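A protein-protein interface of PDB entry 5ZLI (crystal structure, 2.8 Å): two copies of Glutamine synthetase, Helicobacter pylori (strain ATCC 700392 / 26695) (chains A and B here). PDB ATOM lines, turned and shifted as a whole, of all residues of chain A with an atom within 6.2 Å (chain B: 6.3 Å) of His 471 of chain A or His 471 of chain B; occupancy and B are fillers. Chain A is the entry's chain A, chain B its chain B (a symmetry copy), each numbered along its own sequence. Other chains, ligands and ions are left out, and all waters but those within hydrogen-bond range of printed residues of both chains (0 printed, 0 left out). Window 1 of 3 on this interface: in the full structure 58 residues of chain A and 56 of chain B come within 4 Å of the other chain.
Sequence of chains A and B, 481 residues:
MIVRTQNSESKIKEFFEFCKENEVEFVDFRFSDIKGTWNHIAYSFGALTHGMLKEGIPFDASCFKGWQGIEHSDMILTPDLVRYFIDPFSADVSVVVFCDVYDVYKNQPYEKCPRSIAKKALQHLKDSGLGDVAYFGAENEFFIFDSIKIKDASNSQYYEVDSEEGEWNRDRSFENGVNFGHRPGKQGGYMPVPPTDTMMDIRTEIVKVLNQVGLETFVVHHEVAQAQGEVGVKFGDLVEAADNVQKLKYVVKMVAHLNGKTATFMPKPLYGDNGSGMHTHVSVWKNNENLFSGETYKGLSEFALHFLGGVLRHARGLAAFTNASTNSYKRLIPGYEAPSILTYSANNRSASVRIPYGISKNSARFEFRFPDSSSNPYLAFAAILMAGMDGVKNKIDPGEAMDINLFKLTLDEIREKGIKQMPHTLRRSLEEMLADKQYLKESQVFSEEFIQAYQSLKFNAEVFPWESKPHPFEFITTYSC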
ATOM      1  N   GLN A 157      22.725 -32.305   6.282  1.00  0.00           N
ATOM      2  CA  GLN A 157      22.414 -30.991   6.822  1.00  0.00           C
ATOM      3  C   GLN A 157      21.076 -31.055   7.561  1.00  0.00           C
ATOM      4  O   GLN A 157      20.098 -31.580   7.018  1.00  0.00           O
ATOM      5  CB  GLN A 157      22.336 -29.959   5.688  1.00  0.00           C
ATOM      6  CG  GLN A 157      23.609 -29.779   4.872  1.00  0.00           C
ATOM      7  CD  GLN A 157      24.757 -29.216   5.673  1.00  0.00           C
ATOM      8  OE1 GLN A 157      24.591 -28.313   6.489  1.00  0.00           O
ATOM      9  NE2 GLN A 157      25.937 -29.767   5.452  1.00  0.00           N
ATOM     10  N   TYR A 159      18.291 -29.072  10.620  1.00  0.00           N
ATOM     11  CA  TYR A 159      17.877 -28.196  11.709  1.00  0.00           C
ATOM     12  C   TYR A 159      16.486 -28.560  12.174  1.00  0.00           C
ATOM     13  O   TYR A 159      15.673 -29.106  11.428  1.00  0.00           O
ATOM     14  CB  TYR A 159      17.915 -26.702  11.352  1.00  0.00           C
ATOM     15  CG  TYR A 159      16.688 -26.097  10.714  1.00  0.00           C
ATOM     16  CD1 TYR A 159      15.605 -25.683  11.474  1.00  0.00           C
ATOM     17  CD2 TYR A 159      16.636 -25.882   9.352  1.00  0.00           C
ATOM     18  CE1 TYR A 159      14.487 -25.098  10.881  1.00  0.00           C
ATOM     19  CE2 TYR A 159      15.542 -25.297   8.756  1.00  0.00           C
ATOM     20  CZ  TYR A 159      14.467 -24.905   9.523  1.00  0.00           C
ATOM     21  OH  TYR A 159      13.374 -24.317   8.905  1.00  0.00           O
ATOM     22  N   MET A 266      17.085 -14.204  14.715  1.00  0.00           N
ATOM     23  CA  MET A 266      17.397 -14.508  13.331  1.00  0.00           C
ATOM     24  C   MET A 266      16.176 -14.254  12.444  1.00  0.00           C
ATOM     25  O   MET A 266      15.023 -14.403  12.883  1.00  0.00           O
ATOM     26  CB  MET A 266      17.916 -15.955  13.184  1.00  0.00           C
ATOM     27  CG  MET A 266      16.910 -17.095  13.226  1.00  0.00           C
ATOM     28  SD  MET A 266      17.585 -18.774  13.150  1.00  0.00           S
ATOM     29  CE  MET A 266      18.209 -18.757  11.493  1.00  0.00           C
ATOM     30  N   ASN A 327      19.883 -15.828   5.436  1.00  0.00           N
ATOM     31  CA  ASN A 327      18.587 -16.099   6.028  1.00  0.00           C
ATOM     32  C   ASN A 327      17.709 -14.875   5.915  1.00  0.00           C
ATOM     33  O   ASN A 327      16.505 -15.021   5.693  1.00  0.00           O
ATOM     34  CB  ASN A 327      18.786 -16.521   7.494  1.00  0.00           C
ATOM     35  CG  ASN A 327      17.515 -17.032   8.162  1.00  0.00           C
ATOM     36  OD1 ASN A 327      17.031 -16.456   9.141  1.00  0.00           O
ATOM     37  ND2 ASN A 327      16.991 -18.150   7.663  1.00  0.00           N
ATOM     38  N   LYS A 330      15.338 -15.079   3.070  1.00  0.00           N
ATOM     39  CA  LYS A 330      14.249 -16.036   3.223  1.00  0.00           C
ATOM     40  C   LYS A 330      12.996 -15.379   3.794  1.00  0.00           C
ATOM     41  O   LYS A 330      11.893 -15.919   3.632  1.00  0.00           O
ATOM     42  CB  LYS A 330      14.719 -17.178   4.132  1.00  0.00           C
ATOM     43  CG  LYS A 330      16.193 -17.631   3.907  1.00  0.00           C
ATOM     44  CD  LYS A 330      16.336 -18.695   2.824  1.00  0.00           C
ATOM     45  CE  LYS A 330      17.762 -18.797   2.315  1.00  0.00           C
ATOM     46  NZ  LYS A 330      17.954 -20.011   1.440  1.00  0.00           N
ATOM     47  N   PRO A 465      29.307 -20.432   1.906  1.00  0.00           N
ATOM     48  CA  PRO A 465      28.727 -21.641   2.494  1.00  0.00           C
ATOM     49  C   PRO A 465      27.324 -21.932   1.991  1.00  0.00           C
ATOM     50  O   PRO A 465      26.996 -23.088   1.720  1.00  0.00           O
ATOM     51  CB  PRO A 465      28.745 -21.333   3.997  1.00  0.00           C
ATOM     52  CG  PRO A 465      29.817 -20.353   4.178  1.00  0.00           C
ATOM     53  CD  PRO A 465      29.700 -19.478   2.953  1.00  0.00           C
ATOM     54  N   TRP A 466      26.485 -20.911   1.837  1.00  0.00           N
ATOM     55  CA  TRP A 466      25.126 -21.170   1.391  1.00  0.00           C
ATOM     56  C   TRP A 466      25.094 -21.635  -0.054  1.00  0.00           C
ATOM     57  O   TRP A 466      24.273 -22.486  -0.431  1.00  0.00           O
ATOM     58  CB  TRP A 466      24.277 -19.920   1.566  1.00  0.00           C
ATOM     59  CG  TRP A 466      22.881 -20.077   1.101  1.00  0.00           C
ATOM     60  CD1 TRP A 466      21.941 -20.917   1.605  1.00  0.00           C
ATOM     61  CD2 TRP A 466      22.265 -19.387   0.017  1.00  0.00           C
ATOM     62  NE1 TRP A 466      20.761 -20.782   0.909  1.00  0.00           N
ATOM     63  CE2 TRP A 466      20.940 -19.848  -0.075  1.00  0.00           C
ATOM     64  CE3 TRP A 466      22.704 -18.418  -0.880  1.00  0.00           C
ATOM     65  CZ2 TRP A 466      20.048 -19.372  -1.027  1.00  0.00           C
ATOM     66  CZ3 TRP A 466      21.818 -17.945  -1.841  1.00  0.00           C
ATOM     67  CH2 TRP A 466      20.502 -18.419  -1.901  1.00  0.00           C
ATOM     68  N   LYS A 469      26.742 -25.622   0.383  1.00  0.00           N
ATOM     69  CA  LYS A 469      26.252 -26.734   1.176  1.00  0.00           C
ATOM     70  C   LYS A 469      24.877 -27.101   0.648  1.00  0.00           C
ATOM     71  O   LYS A 469      24.002 -26.227   0.585  1.00  0.00           O
ATOM     72  CB  LYS A 469      26.175 -26.365   2.653  1.00  0.00           C
ATOM     73  CG  LYS A 469      27.522 -26.057   3.291  1.00  0.00           C
ATOM     74  CD  LYS A 469      27.385 -25.449   4.673  1.00  0.00           C
ATOM     75  CE  LYS A 469      28.745 -25.105   5.205  1.00  0.00           C
ATOM     76  NZ  LYS A 469      29.584 -26.337   5.356  1.00  0.00           N
ATOM     77  N   PRO A 470      24.657 -28.333   0.209  1.00  0.00           N
ATOM     78  CA  PRO A 470      23.363 -28.693  -0.366  1.00  0.00           C
ATOM     79  C   PRO A 470      22.246 -28.519   0.653  1.00  0.00           C
ATOM     80  O   PRO A 470      22.458 -28.558   1.865  1.00  0.00           O
ATOM     81  CB  PRO A 470      23.544 -30.169  -0.748  1.00  0.00           C
ATOM     82  CG  PRO A 470      25.019 -30.397  -0.723  1.00  0.00           C
ATOM     83  CD  PRO A 470      25.558 -29.488   0.309  1.00  0.00           C
ATOM     84  N   HIS A 471      21.053 -28.305   0.146  1.00  0.00           N
ATOM     85  CA  HIS A 471      19.857 -28.047   0.922  1.00  0.00           C
ATOM     86  C   HIS A 471      18.899 -29.224   0.818  1.00  0.00           C
ATOM     87  O   HIS A 471      18.658 -29.725  -0.291  1.00  0.00           O
ATOM     88  CB  HIS A 471      19.184 -26.770   0.406  1.00  0.00           C
ATOM     89  CG  HIS A 471      18.024 -26.305   1.224  1.00  0.00           C
ATOM     90  ND1 HIS A 471      16.871 -27.046   1.369  1.00  0.00           N
ATOM     91  CD2 HIS A 471      17.799 -25.129   1.852  1.00  0.00           C
ATOM     92  CE1 HIS A 471      16.015 -26.376   2.115  1.00  0.00           C
ATOM     93  NE2 HIS A 471      16.551 -25.203   2.411  1.00  0.00           N
ATOM     94  N   PRO A 472      18.311 -29.662   1.949  1.00  0.00           N
ATOM     95  CA  PRO A 472      17.410 -30.826   1.940  1.00  0.00           C
ATOM     96  C   PRO A 472      16.285 -30.773   0.912  1.00  0.00           C
ATOM     97  O   PRO A 472      15.748 -31.813   0.542  1.00  0.00           O
ATOM     98  CB  PRO A 472      16.841 -30.834   3.368  1.00  0.00           C
ATOM     99  CG  PRO A 472      17.168 -29.471   3.942  1.00  0.00           C
ATOM    100  CD  PRO A 472      18.438 -29.066   3.290  1.00  0.00           C
ATOM    101  N   PHE A 473      15.914 -29.603   0.418  1.00  0.00           N
ATOM    102  CA  PHE A 473      14.824 -29.580  -0.550  1.00  0.00           C
ATOM    103  C   PHE A 473      15.272 -30.039  -1.931  1.00  0.00           C
ATOM    104  O   PHE A 473      14.473 -30.556  -2.719  1.00  0.00           O
ATOM    105  CB  PHE A 473      14.242 -28.181  -0.627  1.00  0.00           C
ATOM    106  CG  PHE A 473      12.972 -28.109  -1.402  1.00  0.00           C
ATOM    107  CD1 PHE A 473      11.818 -28.705  -0.908  1.00  0.00           C
ATOM    108  CD2 PHE A 473      12.900 -27.379  -2.570  1.00  0.00           C
ATOM    109  CE1 PHE A 473      10.623 -28.618  -1.600  1.00  0.00           C
ATOM    110  CE2 PHE A 473      11.725 -27.301  -3.268  1.00  0.00           C
ATOM    111  CZ  PHE A 473      10.577 -27.905  -2.782  1.00  0.00           C
ATOM    112  N   GLU A 474      16.541 -29.861  -2.240  1.00  0.00           N
ATOM    113  CA  GLU A 474      17.050 -30.366  -3.501  1.00  0.00           C
ATOM    114  C   GLU A 474      16.901 -31.879  -3.569  1.00  0.00           C
ATOM    115  O   GLU A 474      16.667 -32.439  -4.646  1.00  0.00           O
ATOM    116  CB  GLU A 474      18.493 -29.891  -3.626  1.00  0.00           C
ATOM    117  CG  GLU A 474      18.539 -28.381  -3.421  1.00  0.00           C
ATOM    118  CD  GLU A 474      19.915 -27.769  -3.356  1.00  0.00           C
ATOM    119  OE1 GLU A 474      20.056 -26.645  -3.883  1.00  0.00           O
ATOM    120  OE2 GLU A 474      20.848 -28.377  -2.795  1.00  0.00           O
ATOM    121  N   PHE A 475      16.912 -32.535  -2.409  1.00  0.00           N
ATOM    122  CA  PHE A 475      16.686 -33.968  -2.350  1.00  0.00           C
ATOM    123  C   PHE A 475      15.230 -34.330  -2.597  1.00  0.00           C
ATOM    124  O   PHE A 475      14.936 -35.430  -3.056  1.00  0.00           O
ATOM    125  CB  PHE A 475      17.128 -34.508  -1.000  1.00  0.00           C
ATOM    126  CG  PHE A 475      18.591 -34.420  -0.781  1.00  0.00           C
ATOM    127  CD1 PHE A 475      19.170 -33.233  -0.379  1.00  0.00           C
ATOM    128  CD2 PHE A 475      19.400 -35.504  -1.036  1.00  0.00           C
ATOM    129  CE1 PHE A 475      20.523 -33.133  -0.192  1.00  0.00           C
ATOM    130  CE2 PHE A 475      20.762 -35.411  -0.849  1.00  0.00           C
ATOM    131  CZ  PHE A 475      21.324 -34.226  -0.422  1.00  0.00           C
ATOM    132  N   ILE A 476      14.292 -33.467  -2.259  1.00  0.00           N
ATOM    133  CA  ILE A 476      12.932 -33.784  -2.649  1.00  0.00           C
ATOM    134  C   ILE A 476      12.772 -33.602  -4.138  1.00  0.00           C
ATOM    135  O   ILE A 476      12.091 -34.396  -4.799  1.00  0.00           O
ATOM    136  CB  ILE A 476      11.935 -32.928  -1.857  1.00  0.00           C
ATOM    137  CG1 ILE A 476      12.021 -33.294  -0.372  1.00  0.00           C
ATOM    138  CG2 ILE A 476      10.531 -33.129  -2.390  1.00  0.00           C
ATOM    139  CD1 ILE A 476      11.474 -32.240   0.520  1.00  0.00           C
ATOM    140  N   ASP B 152      10.879 -31.713   5.224  1.00  0.00           N
ATOM    141  CA  ASP B 152      10.501 -30.339   4.870  1.00  0.00           C
ATOM    142  C   ASP B 152       9.309 -29.979   5.725  1.00  0.00           C
ATOM    143  O   ASP B 152       8.243 -30.589   5.585  1.00  0.00           O
ATOM    144  CB  ASP B 152      10.106 -30.147   3.405  1.00  0.00           C
ATOM    145  CG  ASP B 152       9.829 -28.653   3.063  1.00  0.00           C
ATOM    146  OD1 ASP B 152      10.750 -27.824   3.257  1.00  0.00           O
ATOM    147  OD2 ASP B 152       8.680 -28.285   2.692  1.00  0.00           O
ATOM    148  N   GLN B 157      14.155 -28.440   8.529  1.00  0.00           N
ATOM    149  CA  GLN B 157      14.680 -28.907   7.258  1.00  0.00           C
ATOM    150  C   GLN B 157      15.758 -29.928   7.578  1.00  0.00           C
ATOM    151  O   GLN B 157      16.437 -29.810   8.602  1.00  0.00           O
ATOM    152  CB  GLN B 157      15.239 -27.763   6.409  1.00  0.00           C
ATOM    153  CG  GLN B 157      14.196 -26.773   5.951  1.00  0.00           C
ATOM    154  CD  GLN B 157      13.228 -27.400   4.963  1.00  0.00           C
ATOM    155  OE1 GLN B 157      13.633 -28.136   4.080  1.00  0.00           O
ATOM    156  NE2 GLN B 157      11.949 -27.124   5.125  1.00  0.00           N
ATOM    157  N   TYR B 159      18.164 -33.465   5.744  1.00  0.00           N
ATOM    158  CA  TYR B 159      18.484 -34.573   4.859  1.00  0.00           C
ATOM    159  C   TYR B 159      19.578 -35.430   5.479  1.00  0.00           C
ATOM    160  O   TYR B 159      20.356 -34.992   6.332  1.00  0.00           O
ATOM    161  CB  TYR B 159      18.884 -34.091   3.449  1.00  0.00           C
ATOM    162  CG  TYR B 159      20.333 -33.681   3.238  1.00  0.00           C
ATOM    163  CD1 TYR B 159      21.338 -34.628   3.033  1.00  0.00           C
ATOM    164  CD2 TYR B 159      20.681 -32.341   3.148  1.00  0.00           C
ATOM    165  CE1 TYR B 159      22.651 -34.246   2.808  1.00  0.00           C
ATOM    166  CE2 TYR B 159      21.987 -31.948   2.913  1.00  0.00           C
ATOM    167  CZ  TYR B 159      22.967 -32.907   2.749  1.00  0.00           C
ATOM    168  OH  TYR B 159      24.273 -32.530   2.531  1.00  0.00           O
ATOM    169  N   MET B 266      21.936 -36.794  -8.842  1.00  0.00           N
ATOM    170  CA  MET B 266      21.932 -35.372  -8.474  1.00  0.00           C
ATOM    171  C   MET B 266      23.353 -34.816  -8.341  1.00  0.00           C
ATOM    172  O   MET B 266      24.248 -35.497  -7.833  1.00  0.00           O
ATOM    173  CB  MET B 266      21.145 -35.142  -7.168  1.00  0.00           C
ATOM    174  CG  MET B 266      21.814 -35.550  -5.853  1.00  0.00           C
ATOM    175  SD  MET B 266      20.771 -35.337  -4.372  1.00  0.00           S
ATOM    176  CE  MET B 266      20.701 -33.581  -4.279  1.00  0.00           C
ATOM    177  N   ASN B 327      20.900 -27.332  -7.188  1.00  0.00           N
ATOM    178  CA  ASN B 327      21.901 -28.252  -6.696  1.00  0.00           C
ATOM    179  C   ASN B 327      23.087 -28.325  -7.653  1.00  0.00           C
ATOM    180  O   ASN B 327      24.209 -28.646  -7.242  1.00  0.00           O
ATOM    181  CB  ASN B 327      21.295 -29.625  -6.508  1.00  0.00           C
ATOM    182  CG  ASN B 327      22.165 -30.481  -5.705  1.00  0.00           C
ATOM    183  OD1 ASN B 327      22.690 -31.497  -6.167  1.00  0.00           O
ATOM    184  ND2 ASN B 327      22.346 -30.082  -4.457  1.00  0.00           N
ATOM    185  N   LYS B 330      25.893 -26.082  -6.304  1.00  0.00           N
ATOM    186  CA  LYS B 330      26.737 -26.556  -5.214  1.00  0.00           C
ATOM    187  C   LYS B 330      27.921 -27.370  -5.707  1.00  0.00           C
ATOM    188  O   LYS B 330      28.889 -27.543  -4.967  1.00  0.00           O
ATOM    189  CB  LYS B 330      25.898 -27.376  -4.237  1.00  0.00           C
ATOM    190  CG  LYS B 330      24.564 -26.712  -3.956  1.00  0.00           C
ATOM    191  CD  LYS B 330      24.683 -25.726  -2.784  1.00  0.00           C
ATOM    192  CE  LYS B 330      23.582 -24.689  -2.859  1.00  0.00           C
ATOM    193  NZ  LYS B 330      22.238 -25.253  -3.049  1.00  0.00           N
ATOM    194  N   PRO B 465      11.667 -21.928  -4.077  1.00  0.00           N
ATOM    195  CA  PRO B 465      11.779 -22.756  -2.861  1.00  0.00           C
ATOM    196  C   PRO B 465      13.155 -22.747  -2.191  1.00  0.00           C
ATOM    197  O   PRO B 465      13.235 -22.854  -0.963  1.00  0.00           O
ATOM    198  CB  PRO B 465      11.376 -24.146  -3.359  1.00  0.00           C
ATOM    199  CG  PRO B 465      10.501 -23.883  -4.535  1.00  0.00           C
ATOM    200  CD  PRO B 465      11.155 -22.710  -5.213  1.00  0.00           C
ATOM    201  N   TRP B 466      14.241 -22.743  -2.948  1.00  0.00           N
ATOM    202  CA  TRP B 466      15.567 -22.677  -2.335  1.00  0.00           C
ATOM    203  C   TRP B 466      15.873 -21.296  -1.755  1.00  0.00           C
ATOM    204  O   TRP B 466      16.641 -21.189  -0.784  1.00  0.00           O
ATOM    205  CB  TRP B 466      16.629 -23.074  -3.360  1.00  0.00           C
ATOM    206  CG  TRP B 466      18.039 -23.000  -2.874  1.00  0.00           C
ATOM    207  CD1 TRP B 466      18.624 -23.743  -1.874  1.00  0.00           C
ATOM    208  CD2 TRP B 466      19.049 -22.126  -3.361  1.00  0.00           C
ATOM    209  NE1 TRP B 466      19.948 -23.392  -1.725  1.00  0.00           N
ATOM    210  CE2 TRP B 466      20.229 -22.393  -2.628  1.00  0.00           C
ATOM    211  CE3 TRP B 466      19.076 -21.149  -4.352  1.00  0.00           C
ATOM    212  CZ2 TRP B 466      21.416 -21.711  -2.865  1.00  0.00           C
ATOM    213  CZ3 TRP B 466      20.241 -20.475  -4.578  1.00  0.00           C
ATOM    214  CH2 TRP B 466      21.402 -20.763  -3.845  1.00  0.00           C
ATOM    215  N   LYS B 469      13.233 -21.333   1.667  1.00  0.00           N
ATOM    216  CA  LYS B 469      13.241 -22.318   2.739  1.00  0.00           C
ATOM    217  C   LYS B 469      14.513 -22.185   3.558  1.00  0.00           C
ATOM    218  O   LYS B 469      15.613 -22.173   2.976  1.00  0.00           O
ATOM    219  CB  LYS B 469      13.126 -23.736   2.189  1.00  0.00           C
ATOM    220  CG  LYS B 469      11.775 -24.074   1.608  1.00  0.00           C
ATOM    221  CD  LYS B 469      11.793 -25.412   0.895  1.00  0.00           C
ATOM    222  CE  LYS B 469      10.427 -25.732   0.330  1.00  0.00           C
ATOM    223  NZ  LYS B 469       9.396 -25.915   1.388  1.00  0.00           N
ATOM    224  N   PRO B 470      14.422 -22.020   4.880  1.00  0.00           N
ATOM    225  CA  PRO B 470      15.637 -21.824   5.667  1.00  0.00           C
ATOM    226  C   PRO B 470      16.556 -23.003   5.481  1.00  0.00           C
ATOM    227  O   PRO B 470      16.130 -24.100   5.119  1.00  0.00           O
ATOM    228  CB  PRO B 470      15.134 -21.734   7.116  1.00  0.00           C
ATOM    229  CG  PRO B 470      13.715 -21.393   7.018  1.00  0.00           C
ATOM    230  CD  PRO B 470      13.229 -22.049   5.737  1.00  0.00           C
ATOM    231  N   HIS B 471      17.823 -22.724   5.619  1.00  0.00           N
ATOM    232  CA  HIS B 471      18.898 -23.669   5.475  1.00  0.00           C
ATOM    233  C   HIS B 471      19.594 -23.856   6.819  1.00  0.00           C
ATOM    234  O   HIS B 471      19.925 -22.870   7.490  1.00  0.00           O
ATOM    235  CB  HIS B 471      19.895 -23.174   4.417  1.00  0.00           C
ATOM    236  CG  HIS B 471      20.939 -24.181   4.037  1.00  0.00           C
ATOM    237  ND1 HIS B 471      21.881 -24.652   4.929  1.00  0.00           N
ATOM    238  CD2 HIS B 471      21.222 -24.764   2.847  1.00  0.00           C
ATOM    239  CE1 HIS B 471      22.681 -25.503   4.309  1.00  0.00           C
ATOM    240  NE2 HIS B 471      22.307 -25.584   3.043  1.00  0.00           N
ATOM    241  N   PRO B 472      19.845 -25.080   7.220  1.00  0.00           N
ATOM    242  CA  PRO B 472      20.483 -25.350   8.520  1.00  0.00           C
ATOM    243  C   PRO B 472      21.795 -24.623   8.788  1.00  0.00           C
ATOM    244  O   PRO B 472      22.176 -24.473   9.941  1.00  0.00           O
ATOM    245  CB  PRO B 472      20.735 -26.862   8.460  1.00  0.00           C
ATOM    246  CG  PRO B 472      20.588 -27.221   7.001  1.00  0.00           C
ATOM    247  CD  PRO B 472      19.580 -26.306   6.460  1.00  0.00           C
ATOM    248  N   PHE B 473      22.515 -24.176   7.769  1.00  0.00           N
ATOM    249  CA  PHE B 473      23.764 -23.510   8.095  1.00  0.00           C
ATOM    250  C   PHE B 473      23.500 -22.094   8.583  1.00  0.00           C
ATOM    251  O   PHE B 473      24.253 -21.560   9.410  1.00  0.00           O
ATOM    252  CB  PHE B 473      24.694 -23.487   6.890  1.00  0.00           C
ATOM    253  CG  PHE B 473      26.102 -23.124   7.249  1.00  0.00           C
ATOM    254  CD1 PHE B 473      26.603 -21.864   6.983  1.00  0.00           C
ATOM    255  CD2 PHE B 473      26.912 -24.036   7.923  1.00  0.00           C
ATOM    256  CE1 PHE B 473      27.914 -21.532   7.350  1.00  0.00           C
ATOM    257  CE2 PHE B 473      28.211 -23.713   8.279  1.00  0.00           C
ATOM    258  CZ  PHE B 473      28.717 -22.456   7.994  1.00  0.00           C
ATOM    259  N   GLU B 474      22.407 -21.494   8.122  1.00  0.00           N
ATOM    260  CA  GLU B 474      22.021 -20.193   8.641  1.00  0.00           C
ATOM    261  C   GLU B 474      21.785 -20.269  10.146  1.00  0.00           C
ATOM    262  O   GLU B 474      21.900 -19.258  10.863  1.00  0.00           O
ATOM    263  CB  GLU B 474      20.777 -19.707   7.901  1.00  0.00           C
ATOM    264  CG  GLU B 474      20.945 -19.718   6.397  1.00  0.00           C
ATOM    265  CD  GLU B 474      19.673 -19.352   5.607  1.00  0.00           C
ATOM    266  OE1 GLU B 474      18.529 -19.682   6.010  1.00  0.00           O
ATOM    267  OE2 GLU B 474      19.834 -18.737   4.537  1.00  0.00           O
ATOM    268  N   PHE B 475      21.449 -21.459  10.632  1.00  0.00           N
ATOM    269  CA  PHE B 475      21.287 -21.640  12.060  1.00  0.00           C
ATOM    270  C   PHE B 475      22.621 -21.658  12.783  1.00  0.00           C
ATOM    271  O   PHE B 475      22.716 -21.189  13.912  1.00  0.00           O
ATOM    272  CB  PHE B 475      20.477 -22.903  12.300  1.00  0.00           C
ATOM    273  CG  PHE B 475      19.032 -22.740  11.957  1.00  0.00           C
ATOM    274  CD1 PHE B 475      18.611 -22.693  10.653  1.00  0.00           C
ATOM    275  CD2 PHE B 475      18.091 -22.651  12.955  1.00  0.00           C
ATOM    276  CE1 PHE B 475      17.293 -22.524  10.348  1.00  0.00           C
ATOM    277  CE2 PHE B 475      16.760 -22.488  12.647  1.00  0.00           C
ATOM    278  CZ  PHE B 475      16.365 -22.419  11.335  1.00  0.00           C
ATOM    279  N   ILE B 476      23.674 -22.140  12.144  1.00  0.00           N
ATOM    280  CA  ILE B 476      24.988 -22.044  12.758  1.00  0.00           C
ATOM    281  C   ILE B 476      25.480 -20.604  12.712  1.00  0.00           C
ATOM    282  O   ILE B 476      26.148 -20.124  13.641  1.00  0.00           O
ATOM    283  CB  ILE B 476      25.949 -23.033  12.066  1.00  0.00           C
ATOM    284  CG1 ILE B 476      25.451 -24.448  12.324  1.00  0.00           C
ATOM    285  CG2 ILE B 476      27.373 -22.930  12.573  1.00  0.00           C
ATOM    286  CD1 ILE B 476      26.025 -25.466  11.415  1.00  0.00           C
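His 471 of chain A touches just these residues of chain B: Gln 157 (3.6 Å), Trp 466 (3.8 Å), Lys 469 (3.2 Å), Pro 470 (3.0 Å) and His 471 (3.6 Å).
Of the printed residues of chain B, Ile 476 of chain A touches Asp 152.
Of chain A, only Lys 469, Pro 470 and His 471 come within 4 Å of His 471 of chain B.
Of the printed residues of chain A, Glu 474 of chain B touches Met 266 (3.8 Å), Asn 327 (2.7 Å) and Lys 330 (3.0 Å).
Ile 476 of chain B touches none of the printed residues of chain A.
The nearest residue of chain B that does not touch His 471 of chain A is Tyr 159 of chain B (4.3 Å).
The nearest residue of chain A that does not touch His 471 of chain B is Gln 157 of chain A (4.04 Å).
Phe 475 of chain B touches Tyr 159 of chain A (CZ to CE1, 3.3 Å).
Glu 474 of chain B touches Met 266 of chain A (O to CE, 3.8 Å).
Asn 327 of chain B touches Pro 470 of chain A (ND2 to CB, 3.9 Å).
CD of Lys 330 of chain B touches N of Pro 470 of chain A, 3.97 Å away.
Pro 465 of chain B touches Phe 473 of chain A.
Phe 473 of chain A touches Lys 469 of chain B (CE1 to CE, 3.5 Å).
Hydrophobic or aromatic side chains of chain B that line the printed part of chain A: Tyr 159, Met 266, Pro 465, Trp 466, Pro 470, His 471, Pro 472, Phe 473 and Phe 475.
Hydrophobic or aromatic side chains of chain A within 4 Å of the printed part of chain B: Tyr 159, Met 266, Pro 465, Trp 466, Pro 470, His 471, Pro 472, Phe 473, Phe 475 and Ile 476.
Among the printed residues, Asp or Glu carboxylates within 4 Å of a Lys or Arg side-chain nitrogen of the other chain: Lys 330 of chain A with Glu 474 of chain B (3.8 Å) and Glu 474 of chain A with Lys 330 of chain B (2.7 Å).
The backbone carbonyl oxygen (O) of Gln 157 of chain A is in hydrogen-bond range of the backbone NH (N) of Tyr 159 of chain B (3.0 Å).
N of Tyr 159 of chain A lies within hydrogen-bond range of O of Gln 157 of chain B, 2.8 Å away.
The side-chain amide nitrogen of Asn 327 of chain A sits at hydrogen-bond distance from the side-chain carboxylate of Glu 474 of chain B, at 2.7 Å.
The side-chain amino group (NZ) of Lys 330 of chain A sits at hydrogen-bond distance from the backbone carbonyl oxygen (O) of Trp 466 of chain B (2.8 Å).
The side-chain amino group of Lys 330 of chain A lies within salt-bridge range of the side-chain carboxylate of Glu 474 of chain B, 3.8 Å away.
The backbone carbonyl oxygen (O) of Lys 469 of chain A sits at hydrogen-bond distance from a ring nitrogen (NE2) of His 471 of chain B, 3.1 Å away.
NE2 of His 471 of chain B sits at hydrogen-bond distance from O of Pro 470 of chain A, 3.2 Å away.
A ring nitrogen (NE2) of His 471 of chain A lies within hydrogen-bond range of the backbone carbonyl oxygen (O) of Lys 469 of chain B (3.2 Å).
NE2 of His 471 of chain A lies within hydrogen-bond range of O of Pro 470 of chain B, 3.0 Å away.
OE2 of Glu 474 of chain A sits at hydrogen-bond distance from ND2 of Asn 327 of chain B (2.8 Å).
The side-chain carboxylate (OE1) of Glu 474 of chain A is in salt-bridge range of the side-chain amino group (NZ) of Lys 330 of chain B (2.7 Å).
The backbone NH (N) of His 471 of chain A is in hydrogen-bond range of the side-chain carboxylate (OE2) of Glu 474 of chain A (2.9 Å).
The side-chain amide oxygen of Gln 157 of chain B lies close to the side-chain carboxylate of Asp 152 of chain B (3.0 Å).
OD2 of Asp 152 of chain B is in salt-bridge range of NZ of Lys 469 of chain B.
Met 266 of chain A touches Glu 474 of chain B, but with the chains exchanged Glu 474 of chain A does not touch Met 266 of chain B (4.2 Å).
Asn 327 of chain A touches Glu 474 of chain B, and with the chains exchanged Glu 474 of chain A touches Asn 327 of chain B.
Lys 469 of chain A touches Phe 473 of chain B, and with the chains exchanged Phe 473 of chain A touches Lys 469 of chain B.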
